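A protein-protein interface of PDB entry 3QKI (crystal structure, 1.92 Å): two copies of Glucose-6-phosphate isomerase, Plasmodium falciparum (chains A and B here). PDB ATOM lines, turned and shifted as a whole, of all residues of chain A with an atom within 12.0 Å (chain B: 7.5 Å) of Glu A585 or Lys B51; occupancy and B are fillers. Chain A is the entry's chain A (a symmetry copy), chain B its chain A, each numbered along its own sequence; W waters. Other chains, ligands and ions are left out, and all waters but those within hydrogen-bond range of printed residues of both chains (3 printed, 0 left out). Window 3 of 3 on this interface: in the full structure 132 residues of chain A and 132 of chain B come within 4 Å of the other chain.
O of Leu B48 sits at hydrogen-bond distance from N of Glu A585, at 3.0 Å.
The side-chain hydroxyl (OG) of Ser B54 lies within hydrogen-bond range of the side-chain hydroxyl (OG) of Ser A586 (2.8 Å).
The side-chain hydroxyl (OG) of Ser B69 sits at hydrogen-bond distance from the side-chain hydroxyl (OG) of Ser A586, at 2.6 Å.
OD1 of Asp B477 is in hydrogen-bond range of ND2 of Asn A584, at 2.9 Å.
The side-chain hydroxyl (OG1) of Thr A587 is in hydrogen-bond range of the side-chain carboxylate (OD2) of Asp B477.
The backbone carbonyl oxygen of Asp B50 lies within hydrogen-bond range of the side-chain hydroxyl of Ser B54 (3.4 Å).
NH1 of Arg B53 is in hydrogen-bond range of O of Ser B69 (2.7 Å).
The guanidinium group (NH1) of Arg B70 is in salt-bridge range of the side-chain carboxylate (OD2) of Asp B67 (2.7 Å).
NE of Arg B70 is in salt-bridge range of OD1 of Asp B477, 3.0 Å away.
The backbone NH (N) of Ser A586 sits at hydrogen-bond distance from the side-chain amide oxygen (OD1) of Asn A584, at 2.9 Å.
OE2 of Glu A585 lies within salt-bridge range of NZ of Lys A588, at 3.1 Å.
Asn A584 touches Leu B48.
O of Asn B49 touches CG of Glu A585 (3.7 Å).
OE1 of Glu A585 touches CG of Lys B51, at 3.6 Å.
CB of Glu A585 touches OG of Ser B54, 3.7 Å away.
Ser A586 touches Leu B48.
Ser A586 touches Asp B67 (CB to OD2, 3.6 Å).
Arg B70 touches Ser A586.
CG2 of Thr A587 touches NH2 of Arg B70, at 3.5 Å.
Glu B55 touches Ile A589 (CG to CD1, 3.99 Å).
Leu A590 touches Asp B67.
Glu A585 touches just these residues of chain B: Leu B48, Asn B49, Lys B51 and Ser B54.
Of the printed residues of chain B, Ser A586 touches Leu B48, Ser B54, Asp B67, Ser B69 and Arg B70.
Of the printed residues of chain B, Thr A587 touches Arg B70 and Asp B477.
Of the printed residues of chain B, Leu A590 touches Asp B67 (3.9 Å).
Of chain A, only Glu A585 (3.7 Å) comes within 4 Å of Asn B49.
Lys B51 touches one residue of chain A.
Ser B54 touches just these residues of chain A: Glu A585 (3.7 Å) and Ser A586 (2.8 Å).
Ile B58 touches none of the printed residues of chain A.
The nearest residue of chain A that does not touch Lys B51 is Ile A589 (4.9 Å).
The nearest printed residue of chain B that does not touch Ser A586 is Ile B58 (4.03 Å).
Of the 18 printed residues of chain B, 9 touch a printed residue of chain A.
Of the 16 printed residues of chain A, 6 touch a printed residue of chain B.
Printed residues of chain A that touch a printed residue of chain B: Asn A584, Glu A585, Ser A586, Thr A587, Ile A589 and Leu A590.
Along chain A the printed residues that touch a printed residue of chain B span positions 584 to 590.
Among the printed residues, no Asp or Glu carboxylate lies within 4 Å of a Lys or Arg side-chain nitrogen of the other chain.
No position is printed for both chains.
Water W2 lies within hydrogen-bond range of the side-chain carboxylate of Asp B67 (2.6 Å), the guanidinium group of Arg B70 (2.8 Å) and the backbone carbonyl oxygen of Ser A586 (3.2 Å).
Water W3 lies within hydrogen-bond range of OD2 of Asp B477 (2.7 Å), OG1 of Thr A587 (2.8 Å) and N of Asn A584 (2.9 Å).
Water W1 lies within hydrogen-bond range of the side-chain carboxylate of Glu A585 (2.7 Å) and the backbone carbonyl oxygen of Asn B49 (2.7 Å).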
ATOM      1  N   GLU A 563       7.460  -7.203   2.992  1.00  0.00           N
ATOM      2  CA  GLU A 563       7.892  -5.888   3.487  1.00  0.00           C
ATOM      3  C   GLU A 563       6.723  -4.869   3.421  1.00  0.00           C
ATOM      4  O   GLU A 563       6.531  -4.091   4.372  1.00  0.00           O
ATOM      5  CB  GLU A 563       9.099  -5.393   2.687  1.00  0.00           C
ATOM      6  CG  GLU A 563       9.679  -4.088   3.221  1.00  0.00           C
ATOM      7  CD  GLU A 563      10.844  -3.455   2.484  1.00  0.00           C
ATOM      8  OE1 GLU A 563      11.277  -4.002   1.442  1.00  0.00           O
ATOM      9  OE2 GLU A 563      11.319  -2.395   2.955  1.00  0.00           O
ATOM     10  N   TYR A 567       4.541  -2.960   6.503  1.00  0.00           N
ATOM     11  CA  TYR A 567       4.308  -1.529   6.405  1.00  0.00           C
ATOM     12  C   TYR A 567       2.816  -1.221   6.526  1.00  0.00           C
ATOM     13  O   TYR A 567       2.447  -0.302   7.252  1.00  0.00           O
ATOM     14  CB  TYR A 567       4.887  -0.953   5.107  1.00  0.00           C
ATOM     15  CG  TYR A 567       4.756   0.553   5.043  1.00  0.00           C
ATOM     16  CD1 TYR A 567       5.497   1.374   5.894  1.00  0.00           C
ATOM     17  CD2 TYR A 567       3.867   1.155   4.163  1.00  0.00           C
ATOM     18  CE1 TYR A 567       5.353   2.763   5.865  1.00  0.00           C
ATOM     19  CE2 TYR A 567       3.719   2.541   4.122  1.00  0.00           C
ATOM     20  CZ  TYR A 567       4.472   3.342   4.969  1.00  0.00           C
ATOM     21  OH  TYR A 567       4.332   4.706   4.917  1.00  0.00           O
ATOM     22  N   TYR A 581      11.952   0.227   6.786  1.00  0.00           N
ATOM     23  CA  TYR A 581      11.483   0.329   5.386  1.00  0.00           C
ATOM     24  C   TYR A 581      12.354   1.185   4.510  1.00  0.00           C
ATOM     25  O   TYR A 581      12.785   2.255   4.946  1.00  0.00           O
ATOM     26  CB  TYR A 581      10.011   0.790   5.319  1.00  0.00           C
ATOM     27  CG  TYR A 581       9.121  -0.043   6.223  1.00  0.00           C
ATOM     28  CD1 TYR A 581       8.758  -1.339   5.873  1.00  0.00           C
ATOM     29  CD2 TYR A 581       8.748   0.421   7.484  1.00  0.00           C
ATOM     30  CE1 TYR A 581       8.026  -2.145   6.739  1.00  0.00           C
ATOM     31  CE2 TYR A 581       8.020  -0.376   8.360  1.00  0.00           C
ATOM     32  CZ  TYR A 581       7.660  -1.657   7.983  1.00  0.00           C
ATOM     33  OH  TYR A 581       6.926  -2.432   8.831  1.00  0.00           O
ATOM     34  N   ASN A 582      12.649   0.699   3.289  1.00  0.00           N
ATOM     35  CA  ASN A 582      13.436   1.441   2.316  1.00  0.00           C
ATOM     36  C   ASN A 582      12.769   1.378   0.954  1.00  0.00           C
ATOM     37  O   ASN A 582      13.212   0.645   0.059  1.00  0.00           O
ATOM     38  CB  ASN A 582      14.895   0.978   2.276  1.00  0.00           C
ATOM     39  CG  ASN A 582      15.832   2.060   1.789  1.00  0.00           C
ATOM     40  OD1 ASN A 582      16.441   1.946   0.718  1.00  0.00           O
ATOM     41  ND2 ASN A 582      15.961   3.141   2.561  1.00  0.00           N
ATOM     42  N   PHE A 583      11.652   2.082   0.826  1.00  0.00           N
ATOM     43  CA  PHE A 583      10.898   2.101  -0.421  1.00  0.00           C
ATOM     44  C   PHE A 583      11.484   3.129  -1.361  1.00  0.00           C
ATOM     45  O   PHE A 583      11.946   4.172  -0.900  1.00  0.00           O
ATOM     46  CB  PHE A 583       9.415   2.397  -0.158  1.00  0.00           C
ATOM     47  CG  PHE A 583       8.721   1.335   0.663  1.00  0.00           C
ATOM     48  CD1 PHE A 583       8.704   0.008   0.245  1.00  0.00           C
ATOM     49  CD2 PHE A 583       8.114   1.656   1.867  1.00  0.00           C
ATOM     50  CE1 PHE A 583       8.067  -0.972   1.007  1.00  0.00           C
ATOM     51  CE2 PHE A 583       7.467   0.680   2.622  1.00  0.00           C
ATOM     52  CZ  PHE A 583       7.437  -0.627   2.181  1.00  0.00           C
ATOM     53  N   ASN A 584      11.447   2.866  -2.676  1.00  0.00           N
ATOM     54  CA  ASN A 584      11.936   3.821  -3.660  1.00  0.00           C
ATOM     55  C   ASN A 584      11.000   5.054  -3.708  1.00  0.00           C
ATOM     56  O   ASN A 584       9.920   5.039  -3.102  1.00  0.00           O
ATOM     57  CB  ASN A 584      12.142   3.148  -5.022  1.00  0.00           C
ATOM     58  CG  ASN A 584      10.868   2.755  -5.734  1.00  0.00           C
ATOM     59  OD1 ASN A 584       9.953   3.558  -5.945  1.00  0.00           O
ATOM     60  ND2 ASN A 584      10.766   1.493  -6.111  1.00  0.00           N
ATOM     61  N   GLU A 585      11.413   6.106  -4.415  1.00  0.00           N
ATOM     62  CA  GLU A 585      10.641   7.341  -4.485  1.00  0.00           C
ATOM     63  C   GLU A 585       9.236   7.206  -5.070  1.00  0.00           C
ATOM     64  O   GLU A 585       8.316   7.880  -4.596  1.00  0.00           O
ATOM     65  CB  GLU A 585      11.441   8.452  -5.163  1.00  0.00           C
ATOM     66  CG  GLU A 585      12.717   8.826  -4.430  1.00  0.00           C
ATOM     67  CD  GLU A 585      12.590   9.233  -2.974  1.00  0.00           C
ATOM     68  OE1 GLU A 585      11.624   9.943  -2.612  1.00  0.00           O
ATOM     69  OE2 GLU A 585      13.464   8.822  -2.185  1.00  0.00           O
ATOM     70  N   SER A 586       9.048   6.322  -6.076  1.00  0.00           N
ATOM     71  CA  SER A 586       7.715   6.144  -6.660  1.00  0.00           C
ATOM     72  C   SER A 586       6.786   5.406  -5.727  1.00  0.00           C
ATOM     73  O   SER A 586       5.634   5.835  -5.546  1.00  0.00           O
ATOM     74  CB  SER A 586       7.793   5.412  -7.994  1.00  0.00           C
ATOM     75  OG  SER A 586       8.562   6.186  -8.888  1.00  0.00           O
ATOM     76  N   THR A 587       7.273   4.293  -5.132  1.00  0.00           N
ATOM     77  CA  THR A 587       6.448   3.511  -4.211  1.00  0.00           C
ATOM     78  C   THR A 587       6.002   4.299  -3.011  1.00  0.00           C
ATOM     79  O   THR A 587       4.850   4.146  -2.600  1.00  0.00           O
ATOM     80  CB  THR A 587       6.949   2.102  -3.900  1.00  0.00           C
ATOM     81  OG1 THR A 587       8.325   1.964  -4.245  1.00  0.00           O
ATOM     82  CG2 THR A 587       6.121   1.047  -4.597  1.00  0.00           C
ATOM     83  N   LYS A 588       6.855   5.208  -2.493  1.00  0.00           N
ATOM     84  CA  LYS A 588       6.470   6.083  -1.377  1.00  0.00           C
ATOM     85  C   LYS A 588       5.274   6.972  -1.767  1.00  0.00           C
ATOM     86  O   LYS A 588       4.348   7.119  -0.975  1.00  0.00           O
ATOM     87  CB  LYS A 588       7.653   6.952  -0.906  1.00  0.00           C
ATOM     88  CG  LYS A 588       8.735   6.171  -0.178  1.00  0.00           C
ATOM     89  CD  LYS A 588       9.726   7.113   0.511  1.00  0.00           C
ATOM     90  CE  LYS A 588      10.971   7.362  -0.303  1.00  0.00           C
ATOM     91  NZ  LYS A 588      11.958   8.187   0.439  1.00  0.00           N
ATOM     92  N   ILE A 589       5.263   7.520  -2.989  1.00  0.00           N
ATOM     93  CA  ILE A 589       4.169   8.383  -3.458  1.00  0.00           C
ATOM     94  C   ILE A 589       2.848   7.575  -3.566  1.00  0.00           C
ATOM     95  O   ILE A 589       1.807   8.009  -3.051  1.00  0.00           O
ATOM     96  CB  ILE A 589       4.576   9.122  -4.775  1.00  0.00           C
ATOM     97  CG1 ILE A 589       5.750  10.112  -4.499  1.00  0.00           C
ATOM     98  CG2 ILE A 589       3.377   9.845  -5.443  1.00  0.00           C
ATOM     99  CD1 ILE A 589       6.476  10.661  -5.722  1.00  0.00           C
ATOM    100  N   LEU A 590       2.911   6.375  -4.160  1.00  0.00           N
ATOM    101  CA  LEU A 590       1.716   5.542  -4.316  1.00  0.00           C
ATOM    102  C   LEU A 590       1.223   4.914  -3.030  1.00  0.00           C
ATOM    103  O   LEU A 590       0.016   4.793  -2.852  1.00  0.00           O
ATOM    104  CB  LEU A 590       1.836   4.528  -5.472  1.00  0.00           C
ATOM    105  CG  LEU A 590       1.128   4.984  -6.752  1.00  0.00           C
ATOM    106  CD1 LEU A 590       1.846   6.120  -7.395  1.00  0.00           C
ATOM    107  CD2 LEU A 590       1.055   3.849  -7.784  1.00  0.00           C
ATOM    108  N   LEU A 591       2.141   4.547  -2.121  1.00  0.00           N
ATOM    109  CA  LEU A 591       1.755   4.004  -0.818  1.00  0.00           C
ATOM    110  C   LEU A 591       1.003   5.061  -0.011  1.00  0.00           C
ATOM    111  O   LEU A 591       0.009   4.728   0.639  1.00  0.00           O
ATOM    112  CB  LEU A 591       2.950   3.483  -0.015  1.00  0.00           C
ATOM    113  CG  LEU A 591       3.581   2.163  -0.490  1.00  0.00           C
ATOM    114  CD1 LEU A 591       4.786   1.841   0.333  1.00  0.00           C
ATOM    115  CD2 LEU A 591       2.597   1.007  -0.454  1.00  0.00           C
ATOM    116  N   ASN A 592       1.461   6.341  -0.087  1.00  0.00           N
ATOM    117  CA  ASN A 592       0.820   7.469   0.592  1.00  0.00           C
ATOM    118  C   ASN A 592      -0.598   7.648   0.072  1.00  0.00           C
ATOM    119  O   ASN A 592      -1.501   7.878   0.873  1.00  0.00           O
ATOM    120  CB  ASN A 592       1.604   8.776   0.379  1.00  0.00           C
ATOM    121  CG  ASN A 592       2.860   8.905   1.197  1.00  0.00           C
ATOM    122  OD1 ASN A 592       3.008   8.301   2.274  1.00  0.00           O
ATOM    123  ND2 ASN A 592       3.794   9.716   0.703  1.00  0.00           N
ATOM    124  N   TYR A 593      -0.798   7.529  -1.262  1.00  0.00           N
ATOM    125  CA  TYR A 593      -2.127   7.640  -1.845  1.00  0.00           C
ATOM    126  C   TYR A 593      -2.975   6.437  -1.396  1.00  0.00           C
ATOM    127  O   TYR A 593      -4.080   6.624  -0.892  1.00  0.00           O
ATOM    128  CB  TYR A 593      -2.056   7.750  -3.383  1.00  0.00           C
ATOM    129  CG  TYR A 593      -3.413   7.815  -4.042  1.00  0.00           C
ATOM    130  CD1 TYR A 593      -4.352   8.769  -3.656  1.00  0.00           C
ATOM    131  CD2 TYR A 593      -3.761   6.927  -5.056  1.00  0.00           C
ATOM    132  CE1 TYR A 593      -5.610   8.829  -4.253  1.00  0.00           C
ATOM    133  CE2 TYR A 593      -5.012   6.986  -5.669  1.00  0.00           C
ATOM    134  CZ  TYR A 593      -5.943   7.924  -5.248  1.00  0.00           C
ATOM    135  OH  TYR A 593      -7.193   7.973  -5.815  1.00  0.00           O
ATOM    136  N   TYR A 594      -2.431   5.223  -1.520  1.00  0.00           N
ATOM    137  CA  TYR A 594      -3.140   3.986  -1.157  1.00  0.00           C
ATOM    138  C   TYR A 594      -3.649   4.002   0.303  1.00  0.00           C
ATOM    139  O   TYR A 594      -4.764   3.553   0.583  1.00  0.00           O
ATOM    140  CB  TYR A 594      -2.248   2.734  -1.400  1.00  0.00           C
ATOM    141  CG  TYR A 594      -2.968   1.451  -1.070  1.00  0.00           C
ATOM    142  CD1 TYR A 594      -3.979   0.958  -1.902  1.00  0.00           C
ATOM    143  CD2 TYR A 594      -2.739   0.793   0.137  1.00  0.00           C
ATOM    144  CE1 TYR A 594      -4.701  -0.194  -1.565  1.00  0.00           C
ATOM    145  CE2 TYR A 594      -3.445  -0.361   0.474  1.00  0.00           C
ATOM    146  CZ  TYR A 594      -4.405  -0.868  -0.397  1.00  0.00           C
ATOM    147  OH  TYR A 594      -5.097  -2.011  -0.072  1.00  0.00           O
ATOM    148  N   ASP B  46      18.263   2.891 -10.260  1.00  0.00           N
ATOM    149  CA  ASP B  46      18.888   4.205 -10.104  1.00  0.00           C
ATOM    150  C   ASP B  46      17.900   5.307 -10.372  1.00  0.00           C
ATOM    151  O   ASP B  46      17.783   6.209  -9.547  1.00  0.00           O
ATOM    152  CB  ASP B  46      20.164   4.329 -10.937  1.00  0.00           C
ATOM    153  CG  ASP B  46      21.248   3.405 -10.439  1.00  0.00           C
ATOM    154  OD1 ASP B  46      21.531   3.416  -9.200  1.00  0.00           O
ATOM    155  OD2 ASP B  46      21.795   2.652 -11.254  1.00  0.00           O
ATOM    156  N   TYR B  47      17.085   5.170 -11.447  1.00  0.00           N
ATOM    157  CA  TYR B  47      16.037   6.139 -11.781  1.00  0.00           C
ATOM    158  C   TYR B  47      15.030   6.294 -10.634  1.00  0.00           C
ATOM    159  O   TYR B  47      14.607   7.413 -10.336  1.00  0.00           O
ATOM    160  CB  TYR B  47      15.290   5.712 -13.062  1.00  0.00           C
ATOM    161  CG  TYR B  47      15.920   6.130 -14.375  1.00  0.00           C
ATOM    162  CD1 TYR B  47      16.461   7.401 -14.539  1.00  0.00           C
ATOM    163  CD2 TYR B  47      15.849   5.308 -15.494  1.00  0.00           C
ATOM    164  CE1 TYR B  47      16.991   7.810 -15.763  1.00  0.00           C
ATOM    165  CE2 TYR B  47      16.354   5.711 -16.723  1.00  0.00           C
ATOM    166  CZ  TYR B  47      16.942   6.957 -16.853  1.00  0.00           C
ATOM    167  OH  TYR B  47      17.475   7.349 -18.059  1.00  0.00           O
ATOM    168  N   LEU B  48      14.665   5.168  -9.979  1.00  0.00           N
ATOM    169  CA  LEU B  48      13.702   5.159  -8.871  1.00  0.00           C
ATOM    170  C   LEU B  48      14.170   5.836  -7.566  1.00  0.00           C
ATOM    171  O   LEU B  48      13.371   5.983  -6.642  1.00  0.00           O
ATOM    172  CB  LEU B  48      13.087   3.759  -8.626  1.00  0.00           C
ATOM    173  CG  LEU B  48      12.270   3.218  -9.819  1.00  0.00           C
ATOM    174  CD1 LEU B  48      12.191   1.718  -9.785  1.00  0.00           C
ATOM    175  CD2 LEU B  48      10.898   3.904  -9.959  1.00  0.00           C
ATOM    176  N   ASN B  49      15.433   6.277  -7.514  1.00  0.00           N
ATOM    177  CA  ASN B  49      15.989   7.042  -6.395  1.00  0.00           C
ATOM    178  C   ASN B  49      15.857   8.554  -6.650  1.00  0.00           C
ATOM    179  O   ASN B  49      16.083   9.365  -5.749  1.00  0.00           O
ATOM    180  CB  ASN B  49      17.439   6.644  -6.125  1.00  0.00           C
ATOM    181  CG  ASN B  49      17.540   5.267  -5.519  1.00  0.00           C
ATOM    182  OD1 ASN B  49      16.675   4.832  -4.742  1.00  0.00           O
ATOM    183  ND2 ASN B  49      18.568   4.525  -5.899  1.00  0.00           N
ATOM    184  N   ASP B  50      15.427   8.929  -7.859  1.00  0.00           N
ATOM    185  CA  ASP B  50      15.256  10.329  -8.234  1.00  0.00           C
ATOM    186  C   ASP B  50      13.805  10.727  -7.986  1.00  0.00           C
ATOM    187  O   ASP B  50      12.921  10.384  -8.777  1.00  0.00           O
ATOM    188  CB  ASP B  50      15.683  10.524  -9.703  1.00  0.00           C
ATOM    189  CG  ASP B  50      15.674  11.959 -10.244  1.00  0.00           C
ATOM    190  OD1 ASP B  50      16.260  12.186 -11.330  1.00  0.00           O
ATOM    191  OD2 ASP B  50      15.039  12.843  -9.607  1.00  0.00           O
ATOM    192  N   LYS B  51      13.560  11.459  -6.876  1.00  0.00           N
ATOM    193  CA  LYS B  51      12.217  11.915  -6.507  1.00  0.00           C
ATOM    194  C   LYS B  51      11.621  12.866  -7.565  1.00  0.00           C
ATOM    195  O   LYS B  51      10.410  12.828  -7.800  1.00  0.00           O
ATOM    196  CB  LYS B  51      12.195  12.567  -5.118  1.00  0.00           C
ATOM    197  CG  LYS B  51      10.796  12.812  -4.585  1.00  0.00           C
ATOM    198  CD  LYS B  51      10.779  13.607  -3.281  1.00  0.00           C
ATOM    199  CE  LYS B  51       9.365  13.770  -2.780  1.00  0.00           C
ATOM    200  NZ  LYS B  51       9.330  14.144  -1.343  1.00  0.00           N
ATOM    201  N   ASN B  52      12.461  13.696  -8.193  1.00  0.00           N
ATOM    202  CA  ASN B  52      12.002  14.619  -9.212  1.00  0.00           C
ATOM    203  C   ASN B  52      11.445  13.883 -10.422  1.00  0.00           C
ATOM    204  O   ASN B  52      10.378  14.243 -10.922  1.00  0.00           O
ATOM    205  CB  ASN B  52      13.083  15.593  -9.642  1.00  0.00           C
ATOM    206  CG  ASN B  52      12.408  16.669 -10.406  1.00  0.00           C
ATOM    207  OD1 ASN B  52      11.448  17.282  -9.908  1.00  0.00           O
ATOM    208  ND2 ASN B  52      12.719  16.751 -11.698  1.00  0.00           N
ATOM    209  N   ARG B  53      12.155  12.841 -10.869  1.00  0.00           N
ATOM    210  CA  ARG B  53      11.712  12.023 -12.001  1.00  0.00           C
ATOM    211  C   ARG B  53      10.378  11.341 -11.658  1.00  0.00           C
ATOM    212  O   ARG B  53       9.447  11.381 -12.471  1.00  0.00           O
ATOM    213  CB  ARG B  53      12.793  11.012 -12.388  1.00  0.00           C
ATOM    214  CG  ARG B  53      12.431  10.206 -13.615  1.00  0.00           C
ATOM    215  CD  ARG B  53      13.423   9.121 -13.859  1.00  0.00           C
ATOM    216  NE  ARG B  53      12.963   8.155 -14.875  1.00  0.00           N
ATOM    217  CZ  ARG B  53      12.258   7.057 -14.618  1.00  0.00           C
ATOM    218  NH1 ARG B  53      11.851   6.796 -13.388  1.00  0.00           N
ATOM    219  NH2 ARG B  53      11.922   6.231 -15.602  1.00  0.00           N
ATOM    220  N   SER B  54      10.274  10.780 -10.435  1.00  0.00           N
ATOM    221  CA  SER B  54       9.065  10.097  -9.959  1.00  0.00           C
ATOM    222  C   SER B  54       7.880  11.044  -9.961  1.00  0.00           C
ATOM    223  O   SER B  54       6.815  10.683 -10.469  1.00  0.00           O
ATOM    224  CB  SER B  54       9.270   9.483  -8.575  1.00  0.00           C
ATOM    225  OG  SER B  54      10.200   8.417  -8.683  1.00  0.00           O
ATOM    226  N   GLU B  55       8.086  12.286  -9.473  1.00  0.00           N
ATOM    227  CA  GLU B  55       7.040  13.306  -9.453  1.00  0.00           C
ATOM    228  C   GLU B  55       6.594  13.704 -10.856  1.00  0.00           C
ATOM    229  O   GLU B  55       5.415  13.968 -11.061  1.00  0.00           O
ATOM    230  CB  GLU B  55       7.489  14.519  -8.630  1.00  0.00           C
ATOM    231  CG  GLU B  55       7.410  14.274  -7.135  1.00  0.00           C
ATOM    232  CD  GLU B  55       7.839  15.438  -6.254  1.00  0.00           C
ATOM    233  OE1 GLU B  55       7.459  15.434  -5.061  1.00  0.00           O
ATOM    234  OE2 GLU B  55       8.556  16.343  -6.741  1.00  0.00           O
ATOM    235  N   SER B  56       7.524  13.703 -11.823  1.00  0.00           N
ATOM    236  CA  SER B  56       7.229  14.017 -13.220  1.00  0.00           C
ATOM    237  C   SER B  56       6.502  12.868 -13.931  1.00  0.00           C
ATOM    238  O   SER B  56       5.707  13.139 -14.824  1.00  0.00           O
ATOM    239  CB  SER B  56       8.515  14.308 -13.990  1.00  0.00           C
ATOM    240  OG  SER B  56       9.096  15.526 -13.560  1.00  0.00           O
ATOM    241  N   LEU B  57       6.804  11.611 -13.578  1.00  0.00           N
ATOM    242  CA  LEU B  57       6.252  10.423 -14.267  1.00  0.00           C
ATOM    243  C   LEU B  57       5.025   9.814 -13.623  1.00  0.00           C
ATOM    244  O   LEU B  57       4.507   8.794 -14.094  1.00  0.00           O
ATOM    245  CB  LEU B  57       7.341   9.355 -14.538  1.00  0.00           C
ATOM    246  CG  LEU B  57       8.593   9.795 -15.321  1.00  0.00           C
ATOM    247  CD1 LEU B  57       9.360   8.607 -15.841  1.00  0.00           C
ATOM    248  CD2 LEU B  57       8.250  10.683 -16.468  1.00  0.00           C
ATOM    249  N   ILE B  58       4.550  10.439 -12.550  1.00  0.00           N
ATOM    250  CA  ILE B  58       3.327  10.029 -11.862  1.00  0.00           C
ATOM    251  C   ILE B  58       2.310  11.119 -12.142  1.00  0.00           C
ATOM    252  O   ILE B  58       2.519  12.275 -11.761  1.00  0.00           O
ATOM    253  CB  ILE B  58       3.544   9.719 -10.362  1.00  0.00           C
ATOM    254  CG1 ILE B  58       4.432   8.459 -10.209  1.00  0.00           C
ATOM    255  CG2 ILE B  58       2.193   9.563  -9.635  1.00  0.00           C
ATOM    256  CD1 ILE B  58       5.089   8.261  -8.879  1.00  0.00           C
ATOM    257  N   ASP B  67       1.352   5.735 -12.906  1.00  0.00           N
ATOM    258  CA  ASP B  67       2.768   5.762 -12.593  1.00  0.00           C
ATOM    259  C   ASP B  67       3.581   5.123 -13.732  1.00  0.00           C
ATOM    260  O   ASP B  67       3.597   3.898 -13.893  1.00  0.00           O
ATOM    261  CB  ASP B  67       2.999   5.100 -11.205  1.00  0.00           C
ATOM    262  CG  ASP B  67       4.434   5.018 -10.726  1.00  0.00           C
ATOM    263  OD1 ASP B  67       5.336   5.391 -11.493  1.00  0.00           O
ATOM    264  OD2 ASP B  67       4.662   4.520  -9.585  1.00  0.00           O
ATOM    265  N   SER B  69       6.903   5.624 -13.921  1.00  0.00           N
ATOM    266  CA  SER B  69       8.304   5.695 -13.496  1.00  0.00           C
ATOM    267  C   SER B  69       9.130   4.429 -13.695  1.00  0.00           C
ATOM    268  O   SER B  69      10.359   4.521 -13.788  1.00  0.00           O
ATOM    269  CB  SER B  69       8.426   6.214 -12.062  1.00  0.00           C
ATOM    270  OG  SER B  69       7.842   5.288 -11.166  1.00  0.00           O
ATOM    271  N   ARG B  70       8.485   3.252 -13.769  1.00  0.00           N
ATOM    272  CA  ARG B  70       9.221   2.019 -13.993  1.00  0.00           C
ATOM    273  C   ARG B  70       9.295   1.706 -15.478  1.00  0.00           C
ATOM    274  O   ARG B  70       9.189   0.557 -15.873  1.00  0.00           O
ATOM    275  CB  ARG B  70       8.669   0.844 -13.161  1.00  0.00           C
ATOM    276  CG  ARG B  70       8.745   1.091 -11.668  1.00  0.00           C
ATOM    277  CD  ARG B  70       7.817   0.158 -10.933  1.00  0.00           C
ATOM    278  NE  ARG B  70       7.630   0.584  -9.562  1.00  0.00           N
ATOM    279  CZ  ARG B  70       6.850   1.589  -9.178  1.00  0.00           C
ATOM    280  NH1 ARG B  70       6.163   2.290 -10.077  1.00  0.00           N
ATOM    281  NH2 ARG B  70       6.783   1.927  -7.899  1.00  0.00           N
ATOM    282  N   GLU B  75      13.407  11.741 -18.122  1.00  0.00           N
ATOM    283  CA  GLU B  75      12.415  12.755 -18.487  1.00  0.00           C
ATOM    284  C   GLU B  75      12.737  13.328 -19.880  1.00  0.00           C
ATOM    285  O   GLU B  75      11.824  13.661 -20.639  1.00  0.00           O
ATOM    286  CB  GLU B  75      12.368  13.887 -17.466  1.00  0.00           C
ATOM    287  CG  GLU B  75      11.877  13.454 -16.112  1.00  0.00           C
ATOM    288  CD  GLU B  75      12.414  14.306 -14.979  1.00  0.00           C
ATOM    289  OE1 GLU B  75      13.480  13.960 -14.412  1.00  0.00           O
ATOM    290  OE2 GLU B  75      11.773  15.340 -14.679  1.00  0.00           O
ATOM    291  N   ASP B 477       8.020  -3.212  -8.232  1.00  0.00           N
ATOM    292  CA  ASP B 477       9.371  -2.974  -7.744  1.00  0.00           C
ATOM    293  C   ASP B 477      10.336  -4.134  -8.036  1.00  0.00           C
ATOM    294  O   ASP B 477      11.450  -3.866  -8.460  1.00  0.00           O
ATOM    295  CB  ASP B 477       9.373  -2.605  -6.264  1.00  0.00           C
ATOM    296  CG  ASP B 477       8.840  -1.206  -5.973  1.00  0.00           C
ATOM    297  OD1 ASP B 477       8.728  -0.387  -6.935  1.00  0.00           O
ATOM    298  OD2 ASP B 477       8.533  -0.922  -4.781  1.00  0.00           O
HETATM  299  O   HOH W   1      16.015   8.788  -3.085  1.00  0.00           O
HETATM  300  O   HOH W   2       4.517   3.369  -7.264  1.00  0.00           O
HETATM  301  O   HOH W   3      10.254   0.260  -3.088  1.00  0.00           O
